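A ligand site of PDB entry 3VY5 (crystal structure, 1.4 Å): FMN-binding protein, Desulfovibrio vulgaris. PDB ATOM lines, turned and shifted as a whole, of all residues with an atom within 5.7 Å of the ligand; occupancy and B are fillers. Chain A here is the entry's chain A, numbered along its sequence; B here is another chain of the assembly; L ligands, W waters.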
ATOM      1  N   VAL A  15     -15.133  29.974  18.950  1.00  0.00           N
ATOM      2  CA  VAL A  15     -13.866  29.613  19.569  1.00  0.00           C
ATOM      3  C   VAL A  15     -12.900  30.804  19.559  1.00  0.00           C
ATOM      4  O   VAL A  15     -12.686  31.436  18.529  1.00  0.00           O
ATOM      5  CB  VAL A  15     -13.245  28.409  18.826  1.00  0.00           C
ATOM      6  CG1 VAL A  15     -11.844  28.102  19.341  1.00  0.00           C
ATOM      7  CG2 VAL A  15     -14.161  27.183  18.933  1.00  0.00           C
ATOM      8  N   HIS A  27       2.828  28.976  21.360  1.00  0.00           N
ATOM      9  CA  HIS A  27       1.810  28.074  21.885  1.00  0.00           C
ATOM     10  C   HIS A  27       0.453  28.689  21.592  1.00  0.00           C
ATOM     11  O   HIS A  27       0.338  29.903  21.437  1.00  0.00           O
ATOM     12  CB  HIS A  27       2.006  27.782  23.375  1.00  0.00           C
ATOM     13  CG  HIS A  27       1.178  26.628  23.861  1.00  0.00           C
ATOM     14  ND1 HIS A  27       1.079  25.446  23.145  1.00  0.00           N
ATOM     15  CD2 HIS A  27       0.393  26.478  24.952  1.00  0.00           C
ATOM     16  CE1 HIS A  27       0.277  24.618  23.798  1.00  0.00           C
ATOM     17  NE2 HIS A  27      -0.141  25.223  24.893  1.00  0.00           N
ATOM     18  N   LEU A  28      -0.561  27.844  21.494  1.00  0.00           N
ATOM     19  CA  LEU A  28      -1.889  28.300  21.089  1.00  0.00           C
ATOM     20  C   LEU A  28      -2.923  27.478  21.840  1.00  0.00           C
ATOM     21  O   LEU A  28      -2.890  26.244  21.779  1.00  0.00           O
ATOM     22  CB  LEU A  28      -2.051  28.143  19.574  1.00  0.00           C
ATOM     23  CG  LEU A  28      -3.308  28.727  18.904  1.00  0.00           C
ATOM     24  CD1 LEU A  28      -3.378  30.230  19.162  1.00  0.00           C
ATOM     25  CD2 LEU A  28      -3.312  28.426  17.414  1.00  0.00           C
ATOM     26  N   VAL A  29      -3.788  28.172  22.580  1.00  0.00           N
ATOM     27  CA  VAL A  29      -4.878  27.535  23.323  1.00  0.00           C
ATOM     28  C   VAL A  29      -6.190  28.265  23.043  1.00  0.00           C
ATOM     29  O   VAL A  29      -6.222  29.294  22.341  1.00  0.00           O
ATOM     30  CB  VAL A  29      -4.601  27.483  24.844  1.00  0.00           C
ATOM     31  CG1 VAL A  29      -3.348  26.645  25.141  1.00  0.00           C
ATOM     32  CG2 VAL A  29      -4.507  28.885  25.466  1.00  0.00           C
ATOM     33  N   ASN A  30      -7.269  27.739  23.615  1.00  0.00           N
ATOM     34  CA  ASN A  30      -8.611  28.225  23.323  1.00  0.00           C
ATOM     35  C   ASN A  30      -9.459  28.501  24.547  1.00  0.00           C
ATOM     36  O   ASN A  30      -9.195  28.003  25.641  1.00  0.00           O
ATOM     37  CB  ASN A  30      -9.340  27.225  22.419  1.00  0.00           C
ATOM     38  CG  ASN A  30      -8.618  26.984  21.134  1.00  0.00           C
ATOM     39  OD1 ASN A  30      -8.114  25.881  20.896  1.00  0.00           O
ATOM     40  ND2 ASN A  30      -8.540  28.004  20.288  1.00  0.00           N
ATOM     41  N   THR A  31     -10.481  29.334  24.328  1.00  0.00           N
ATOM     42  CA  THR A  31     -11.630  29.405  25.209  1.00  0.00           C
ATOM     43  C   THR A  31     -12.867  29.618  24.330  1.00  0.00           C
ATOM     44  O   THR A  31     -12.761  29.622  23.110  1.00  0.00           O
ATOM     45  CB  THR A  31     -11.458  30.476  26.313  1.00  0.00           C
ATOM     46  OG1 THR A  31     -12.519  30.346  27.270  1.00  0.00           O
ATOM     47  CG2 THR A  31     -11.452  31.902  25.755  1.00  0.00           C
ATOM     48  N   TRP A  32     -14.026  29.777  24.962  1.00  0.00           N
ATOM     49  CA  TRP A  32     -15.263  30.101  24.244  1.00  0.00           C
ATOM     50  C   TRP A  32     -15.550  31.589  24.367  1.00  0.00           C
ATOM     51  O   TRP A  32     -15.320  32.184  25.423  1.00  0.00           O
ATOM     52  CB  TRP A  32     -16.443  29.322  24.822  1.00  0.00           C
ATOM     53  CG  TRP A  32     -16.359  27.841  24.620  1.00  0.00           C
ATOM     54  CD1 TRP A  32     -16.066  26.902  25.561  1.00  0.00           C
ATOM     55  CD2 TRP A  32     -16.581  27.136  23.395  1.00  0.00           C
ATOM     56  NE1 TRP A  32     -16.081  25.650  24.999  1.00  0.00           N
ATOM     57  CE2 TRP A  32     -16.416  25.757  23.678  1.00  0.00           C
ATOM     58  CE3 TRP A  32     -16.924  27.524  22.092  1.00  0.00           C
ATOM     59  CZ2 TRP A  32     -16.551  24.771  22.686  1.00  0.00           C
ATOM     60  CZ3 TRP A  32     -17.073  26.536  21.115  1.00  0.00           C
ATOM     61  CH2 TRP A  32     -16.881  25.181  21.425  1.00  0.00           C
ATOM     62  N   TYR A  35     -17.506  32.771  27.319  1.00  0.00           N
ATOM     63  CA  TYR A  35     -16.801  32.785  28.601  1.00  0.00           C
ATOM     64  C   TYR A  35     -16.082  34.102  28.894  1.00  0.00           C
ATOM     65  O   TYR A  35     -15.720  34.349  30.042  1.00  0.00           O
ATOM     66  CB  TYR A  35     -15.748  31.682  28.644  1.00  0.00           C
ATOM     67  CG  TYR A  35     -16.237  30.251  28.748  1.00  0.00           C
ATOM     68  CD1 TYR A  35     -17.590  29.902  28.627  1.00  0.00           C
ATOM     69  CD2 TYR A  35     -15.309  29.217  28.915  1.00  0.00           C
ATOM     70  CE1 TYR A  35     -17.990  28.562  28.713  1.00  0.00           C
ATOM     71  CE2 TYR A  35     -15.697  27.897  28.987  1.00  0.00           C
ATOM     72  CZ  TYR A  35     -17.039  27.580  28.879  1.00  0.00           C
ATOM     73  OH  TYR A  35     -17.425  26.251  28.965  1.00  0.00           O
ATOM     74  N   VAL A  46     -10.534  35.524  31.202  1.00  0.00           N
ATOM     75  CA  VAL A  46     -10.771  34.167  30.711  1.00  0.00           C
ATOM     76  C   VAL A  46     -10.717  33.204  31.892  1.00  0.00           C
ATOM     77  O   VAL A  46      -9.774  33.251  32.671  1.00  0.00           O
ATOM     78  CB  VAL A  46      -9.660  33.759  29.707  1.00  0.00           C
ATOM     79  CG1 VAL A  46      -9.853  32.327  29.208  1.00  0.00           C
ATOM     80  CG2 VAL A  46      -9.580  34.737  28.529  1.00  0.00           C
ATOM     81  N   PRO A  47     -11.727  32.330  32.055  1.00  0.00           N
ATOM     82  CA  PRO A  47     -11.628  31.311  33.123  1.00  0.00           C
ATOM     83  C   PRO A  47     -10.571  30.257  32.762  1.00  0.00           C
ATOM     84  O   PRO A  47     -10.581  29.727  31.657  1.00  0.00           O
ATOM     85  CB  PRO A  47     -13.025  30.687  33.167  1.00  0.00           C
ATOM     86  CG  PRO A  47     -13.562  30.862  31.759  1.00  0.00           C
ATOM     87  CD  PRO A  47     -12.965  32.181  31.264  1.00  0.00           C
ATOM     88  N   VAL A  48      -9.673  29.978  33.702  1.00  0.00           N
ATOM     89  CA  VAL A  48      -8.561  29.042  33.473  1.00  0.00           C
ATOM     90  C   VAL A  48      -8.801  27.722  34.206  1.00  0.00           C
ATOM     91  O   VAL A  48      -8.862  27.692  35.439  1.00  0.00           O
ATOM     92  CB  VAL A  48      -7.213  29.654  33.904  1.00  0.00           C
ATOM     93  CG1 VAL A  48      -6.081  28.629  33.768  1.00  0.00           C
ATOM     94  CG2 VAL A  48      -6.910  30.899  33.071  1.00  0.00           C
ATOM     95  N   GLY A  49      -8.927  26.638  33.434  1.00  0.00           N
ATOM     96  CA  GLY A  49      -8.948  25.281  33.998  1.00  0.00           C
ATOM     97  C   GLY A  49      -7.573  24.645  33.866  1.00  0.00           C
ATOM     98  O   GLY A  49      -6.953  24.245  34.849  1.00  0.00           O
ATOM     99  N   GLY A  50      -7.084  24.591  32.629  1.00  0.00           N
ATOM    100  CA  GLY A  50      -5.755  24.070  32.327  1.00  0.00           C
ATOM    101  C   GLY A  50      -4.789  25.220  32.176  1.00  0.00           C
ATOM    102  O   GLY A  50      -4.407  25.841  33.172  1.00  0.00           O
ATOM    103  N   MET A  51      -4.391  25.488  30.939  1.00  0.00           N
ATOM    104  CA  MET A  51      -3.474  26.582  30.585  1.00  0.00           C
ATOM    105  C   MET A  51      -2.194  26.615  31.419  1.00  0.00           C
ATOM    106  O   MET A  51      -1.701  27.677  31.792  1.00  0.00           O
ATOM    107  CB  MET A  51      -4.204  27.931  30.608  1.00  0.00           C
ATOM    108  CG  MET A  51      -5.370  27.989  29.629  1.00  0.00           C
ATOM    109  SD  MET A  51      -5.863  29.684  29.303  1.00  0.00           S
ATOM    110  CE  MET A  51      -7.276  29.434  28.227  1.00  0.00           C
ATOM    111  N   HIS A  52      -1.658  25.428  31.711  1.00  0.00           N
ATOM    112  CA  HIS A  52      -0.424  25.345  32.491  1.00  0.00           C
ATOM    113  C   HIS A  52       0.782  25.743  31.654  1.00  0.00           C
ATOM    114  O   HIS A  52       1.657  26.465  32.133  1.00  0.00           O
ATOM    115  CB  HIS A  52      -0.263  23.958  33.100  1.00  0.00           C
ATOM    116  CG  HIS A  52      -1.253  23.665  34.177  1.00  0.00           C
ATOM    117  ND1 HIS A  52      -1.187  24.243  35.422  1.00  0.00           N
ATOM    118  CD2 HIS A  52      -2.338  22.853  34.194  1.00  0.00           C
ATOM    119  CE1 HIS A  52      -2.192  23.805  36.169  1.00  0.00           C
ATOM    120  NE2 HIS A  52      -2.905  22.969  35.432  1.00  0.00           N
ATOM    121  N   LYS A  53       0.825  25.278  30.412  1.00  0.00           N
ATOM    122  CA  LYS A  53       1.901  25.672  29.508  1.00  0.00           C
ATOM    123  C   LYS A  53       1.787  27.167  29.201  1.00  0.00           C
ATOM    124  O   LYS A  53       2.782  27.909  29.244  1.00  0.00           O
ATOM    125  CB  LYS A  53       1.847  24.844  28.222  1.00  0.00           C
ATOM    126  CG  LYS A  53       3.176  24.673  27.528  1.00  0.00           C
ATOM    127  CD  LYS A  53       3.487  25.808  26.569  1.00  0.00           C
ATOM    128  CE  LYS A  53       4.512  25.341  25.547  1.00  0.00           C
ATOM    129  NZ  LYS A  53       4.971  26.442  24.654  1.00  0.00           N
ATOM    130  N   THR A  54       0.564  27.606  28.921  1.00  0.00           N
ATOM    131  CA  THR A  54       0.283  29.002  28.655  1.00  0.00           C
ATOM    132  C   THR A  54       0.720  29.881  29.837  1.00  0.00           C
ATOM    133  O   THR A  54       1.340  30.933  29.627  1.00  0.00           O
ATOM    134  CB  THR A  54      -1.218  29.179  28.349  1.00  0.00           C
ATOM    135  OG1 THR A  54      -1.505  28.487  27.132  1.00  0.00           O
ATOM    136  CG2 THR A  54      -1.594  30.636  28.191  1.00  0.00           C
ATOM    137  N   GLU A  55       0.419  29.453  31.066  1.00  0.00           N
ATOM    138  CA  GLU A  55       0.818  30.217  32.244  1.00  0.00           C
ATOM    139  C   GLU A  55       2.340  30.333  32.391  1.00  0.00           C
ATOM    140  O   GLU A  55       2.857  31.417  32.692  1.00  0.00           O
ATOM    141  CB  GLU A  55       0.207  29.635  33.525  1.00  0.00           C
ATOM    142  CG  GLU A  55       0.520  30.490  34.754  1.00  0.00           C
ATOM    143  CD  GLU A  55      -0.162  30.031  36.022  1.00  0.00           C
ATOM    144  OE1 GLU A  55      -0.791  28.947  36.028  1.00  0.00           O
ATOM    145  OE2 GLU A  55      -0.041  30.764  37.031  1.00  0.00           O
ATOM    146  N   TRP A 106     -14.812  25.056  37.780  1.00  0.00           N
ATOM    147  CA  TRP A 106     -13.617  24.358  37.335  1.00  0.00           C
ATOM    148  C   TRP A 106     -12.415  25.293  37.166  1.00  0.00           C
ATOM    149  O   TRP A 106     -11.297  24.830  36.919  1.00  0.00           O
ATOM    150  CB  TRP A 106     -13.896  23.627  36.012  1.00  0.00           C
ATOM    151  CG  TRP A 106     -14.582  24.482  34.970  1.00  0.00           C
ATOM    152  CD1 TRP A 106     -15.911  24.526  34.703  1.00  0.00           C
ATOM    153  CD2 TRP A 106     -13.961  25.399  34.060  1.00  0.00           C
ATOM    154  NE1 TRP A 106     -16.179  25.407  33.684  1.00  0.00           N
ATOM    155  CE2 TRP A 106     -14.990  25.946  33.257  1.00  0.00           C
ATOM    156  CE3 TRP A 106     -12.638  25.793  33.815  1.00  0.00           C
ATOM    157  CZ2 TRP A 106     -14.744  26.883  32.259  1.00  0.00           C
ATOM    158  CZ3 TRP A 106     -12.390  26.720  32.816  1.00  0.00           C
ATOM    159  CH2 TRP A 106     -13.432  27.256  32.041  1.00  0.00           C
ATOM    160  N   LEU B  68      -9.149  25.188  15.994  1.00  0.00           N
ATOM    161  CA  LEU B  68     -10.498  25.349  15.457  1.00  0.00           C
ATOM    162  C   LEU B  68     -11.411  24.480  16.304  1.00  0.00           C
ATOM    163  O   LEU B  68     -10.964  23.567  16.993  1.00  0.00           O
ATOM    164  CB  LEU B  68     -10.586  24.969  13.977  1.00  0.00           C
ATOM    165  CG  LEU B  68     -10.555  23.482  13.615  1.00  0.00           C
ATOM    166  CD1 LEU B  68     -11.100  23.274  12.217  1.00  0.00           C
ATOM    167  CD2 LEU B  68      -9.149  22.891  13.750  1.00  0.00           C
ATOM    168  N   GLY B  69     -12.704  24.772  16.246  1.00  0.00           N
ATOM    169  CA  GLY B  69     -13.657  23.998  17.037  1.00  0.00           C
ATOM    170  C   GLY B  69     -15.078  24.324  16.628  1.00  0.00           C
ATOM    171  O   GLY B  69     -15.339  25.105  15.716  1.00  0.00           O
ATOM    172  N   THR B  81     -16.379  21.129  21.093  1.00  0.00           N
ATOM    173  CA  THR B  81     -15.043  20.540  21.053  1.00  0.00           C
ATOM    174  C   THR B  81     -14.140  21.358  20.150  1.00  0.00           C
ATOM    175  O   THR B  81     -14.589  22.291  19.462  1.00  0.00           O
ATOM    176  CB  THR B  81     -15.074  19.066  20.579  1.00  0.00           C
ATOM    177  OG1 THR B  81     -13.816  18.440  20.860  1.00  0.00           O
ATOM    178  CG2 THR B  81     -15.382  18.943  19.082  1.00  0.00           C
ATOM    179  N   GLY B  82     -12.871  21.003  20.153  1.00  0.00           N
ATOM    180  CA  GLY B  82     -11.938  21.603  19.230  1.00  0.00           C
ATOM    181  C   GLY B  82     -10.615  20.892  19.249  1.00  0.00           C
ATOM    182  O   GLY B  82     -10.431  19.920  19.988  1.00  0.00           O
ATOM    183  N   PHE B  83      -9.691  21.400  18.433  1.00  0.00           N
ATOM    184  CA  PHE B  83      -8.424  20.722  18.113  1.00  0.00           C
ATOM    185  C   PHE B  83      -7.247  21.685  18.128  1.00  0.00           C
ATOM    186  O   PHE B  83      -7.377  22.835  17.719  1.00  0.00           O
ATOM    187  CB  PHE B  83      -8.492  20.063  16.734  1.00  0.00           C
ATOM    188  CG  PHE B  83      -9.342  18.843  16.712  1.00  0.00           C
ATOM    189  CD1 PHE B  83     -10.717  18.944  16.531  1.00  0.00           C
ATOM    190  CD2 PHE B  83      -8.779  17.588  16.927  1.00  0.00           C
ATOM    191  CE1 PHE B  83     -11.525  17.810  16.570  1.00  0.00           C
ATOM    192  CE2 PHE B  83      -9.573  16.456  16.966  1.00  0.00           C
ATOM    193  CZ  PHE B  83     -10.942  16.567  16.777  1.00  0.00           C
ATOM    194  N   THR B 121      -8.693  18.804  22.212  1.00  0.00           N
ATOM    195  CA  THR B 121      -8.332  19.424  23.491  1.00  0.00           C
ATOM    196  C   THR B 121      -9.548  19.719  24.372  1.00  0.00           C
ATOM    197  O   THR B 121      -9.427  20.382  25.402  1.00  0.00           O
ATOM    198  CB  THR B 121      -7.540  20.716  23.259  1.00  0.00           C
ATOM    199  OG1 THR B 121      -8.208  21.493  22.267  1.00  0.00           O
ATOM    200  CG2 THR B 121      -6.127  20.415  22.784  1.00  0.00           C
ATOM    201  N   LEU B 122     -10.723  19.227  23.963  1.00  0.00           N
ATOM    202  CA  LEU B 122     -11.943  19.390  24.732  1.00  0.00           C
ATOM    203  C   LEU B 122     -12.860  18.202  24.485  1.00  0.00           C
ATOM    204  O   LEU B 122     -12.964  17.742  23.339  1.00  0.00           O
ATOM    205  CB  LEU B 122     -12.644  20.700  24.366  1.00  0.00           C
ATOM    206  CG  LEU B 122     -13.950  21.064  25.085  1.00  0.00           C
ATOM    207  CD1 LEU B 122     -13.741  21.236  26.578  1.00  0.00           C
ATOM    208  CD2 LEU B 122     -14.521  22.347  24.454  1.00  0.00           C
ATOM    209  OXT LEU B 122     -13.518  17.703  25.414  1.00  0.00           O
HETATM  210  N1  LIG L   1      -8.974  25.620  28.740  1.00  0.00           N
HETATM  211  C1  LIG L   1      -9.129  26.485  29.805  1.00  0.00           C
HETATM  212  O1  LIG L   1      -8.301  26.510  30.722  1.00  0.00           O
HETATM  213  N2  LIG L   1     -10.214  27.373  29.835  1.00  0.00           N
HETATM  214  C2  LIG L   1     -11.170  27.384  28.829  1.00  0.00           C
HETATM  215  O2  LIG L   1     -12.109  28.187  28.905  1.00  0.00           O
HETATM  216  C3  LIG L   1     -11.025  26.488  27.778  1.00  0.00           C
HETATM  217  N3  LIG L   1     -11.949  26.462  26.743  1.00  0.00           N
HETATM  218  C4  LIG L   1     -11.695  25.719  25.604  1.00  0.00           C
HETATM  219  C5  LIG L   1     -12.533  25.873  24.501  1.00  0.00           C
HETATM  220  C6  LIG L   1     -12.295  25.138  23.348  1.00  0.00           C
HETATM  221  C7  LIG L   1     -13.218  25.322  22.141  1.00  0.00           C
HETATM  222  C8  LIG L   1     -11.218  24.249  23.297  1.00  0.00           C
HETATM  223  C9  LIG L   1     -10.937  23.427  22.037  1.00  0.00           C
HETATM  224  C10 LIG L   1     -10.373  24.106  24.392  1.00  0.00           C
HETATM  225  C11 LIG L   1     -10.610  24.831  25.560  1.00  0.00           C
HETATM  226  N4  LIG L   1      -9.748  24.730  26.675  1.00  0.00           N
HETATM  227  C12 LIG L   1      -9.933  25.601  27.741  1.00  0.00           C
HETATM  228  C13 LIG L   1      -8.515  23.908  26.626  1.00  0.00           C
HETATM  229  C14 LIG L   1      -7.297  24.783  26.259  1.00  0.00           C
HETATM  230  O3  LIG L   1      -7.361  25.201  24.892  1.00  0.00           O
HETATM  231  C15 LIG L   1      -5.959  24.065  26.511  1.00  0.00           C
HETATM  232  O4  LIG L   1      -5.886  22.902  25.684  1.00  0.00           O
HETATM  233  C16 LIG L   1      -5.778  23.640  27.974  1.00  0.00           C
HETATM  234  O5  LIG L   1      -6.180  24.698  28.867  1.00  0.00           O
HETATM  235  C17 LIG L   1      -4.304  23.310  28.253  1.00  0.00           C
HETATM  236  O6  LIG L   1      -3.534  24.509  28.143  1.00  0.00           O
HETATM  237  P1  LIG L   1      -1.942  24.491  27.985  1.00  0.00           P
HETATM  238  O7  LIG L   1      -1.572  23.739  26.652  1.00  0.00           O
HETATM  239  O8  LIG L   1      -1.347  23.667  29.221  1.00  0.00           O
HETATM  240  O9  LIG L   1      -1.476  25.900  28.010  1.00  0.00           O
HETATM  241  O   HOH W   1      -2.519  22.404  31.189  1.00  0.00           O
HETATM  242  O   HOH W   2      -3.325  22.803  24.806  1.00  0.00           O
HETATM  243  O   HOH W   3      -8.257  22.204  29.867  1.00  0.00           O
HETATM  244  O   HOH W   4     -10.416  21.304  27.849  1.00  0.00           O
HETATM  245  O   HOH W   5      -7.106  23.918  22.505  1.00  0.00           O
HETATM  246  O   HOH W   6      -0.299  21.590  25.948  1.00  0.00           O
HETATM  247  O   HOH W   7      -0.849  21.054  28.996  1.00  0.00           O
HETATM  248  O   HOH W   8      -6.458  20.421  26.804  1.00  0.00           O
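The backbone NH of Asn 30 sits at hydrogen-bond distance from an oxygen (O3) of the ligand (2.8 Å).
A nitrogen (N2) of the ligand sits at hydrogen-bond distance from the backbone carbonyl oxygen of Pro 47, at 3.0 Å.
N of Lys 53 sits at hydrogen-bond distance from O8 of the ligand, 3.0 Å away.
The backbone NH (N) of Met 51 sits at hydrogen-bond distance from an oxygen (O5) of the ligand, 2.8 Å away.
An oxygen (O9) of the ligand lies within hydrogen-bond range of the backbone NH (N) of Thr 54.
N of Gly 49 is in hydrogen-bond range of O1 of the ligand.
O2 of the ligand is in hydrogen-bond range of OG1 of Thr 31 (2.7 Å).
N of Gly 50 sits at hydrogen-bond distance from O1 of the ligand, at 3.0 Å.
The side-chain hydroxyl (OG1) of Thr 54 sits at hydrogen-bond distance from an oxygen (O9) of the ligand (2.7 Å).
An oxygen (O3) of the ligand sits close to the backbone carbonyl oxygen (O) of Asn 30 (3.4 Å).
A ring nitrogen (NE2) of His 27 sits at hydrogen-bond distance from an oxygen (O7) of the ligand (2.7 Å).
O8 of the ligand sits at hydrogen-bond distance from N of His 52.
O of Leu 122 of chain B lies within hydrogen-bond range of OG1 of Thr 81 of chain B (2.7 Å).
The backbone carbonyl oxygen (O) of Gly 82 of chain B sits at hydrogen-bond distance from the backbone NH (N) of Thr 121 of chain B, 3.0 Å away.
Val 15 touches the ligand.
Val 29 touches the ligand (CG1 to O9, 3.5 Å).
CZ2 of Trp 32 touches C7 of the ligand, at 3.4 Å.
CD2 of Tyr 35 touches O2 of the ligand (3.4 Å).
Val 48 touches the ligand (C to O1, 3.7 Å).
CH2 of Trp 106 touches O2 of the ligand, 3.5 Å away.
CA of Gly 82 of chain B touches C9 of the ligand, at 3.5 Å.
OG1 of Thr 121 of chain B touches C9 of the ligand, 3.4 Å away.
Leu 122 of chain B touches the ligand (CD2 to C6, 3.7 Å).
Hydrophobic or aromatic side chains that line the ligand: Val 15, His 27, Val 29, Trp 32, Tyr 35, Met 51, Trp 106 and Leu 122 of chain B.
Water W1 lies within hydrogen-bond range of an oxygen (O8) of the ligand and the backbone NH of His 52.
Water W5 lies within hydrogen-bond range of OG1 of Thr 121 of chain B (2.7 Å), O3 of the ligand (2.7 Å) and OD1 of Asn 30 (2.7 Å).
Water W8 lies within hydrogen-bond range of an oxygen (O4) of the ligand (2.8 Å) and the backbone carbonyl oxygen (O) of Thr 121 of chain B (3.3 Å).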
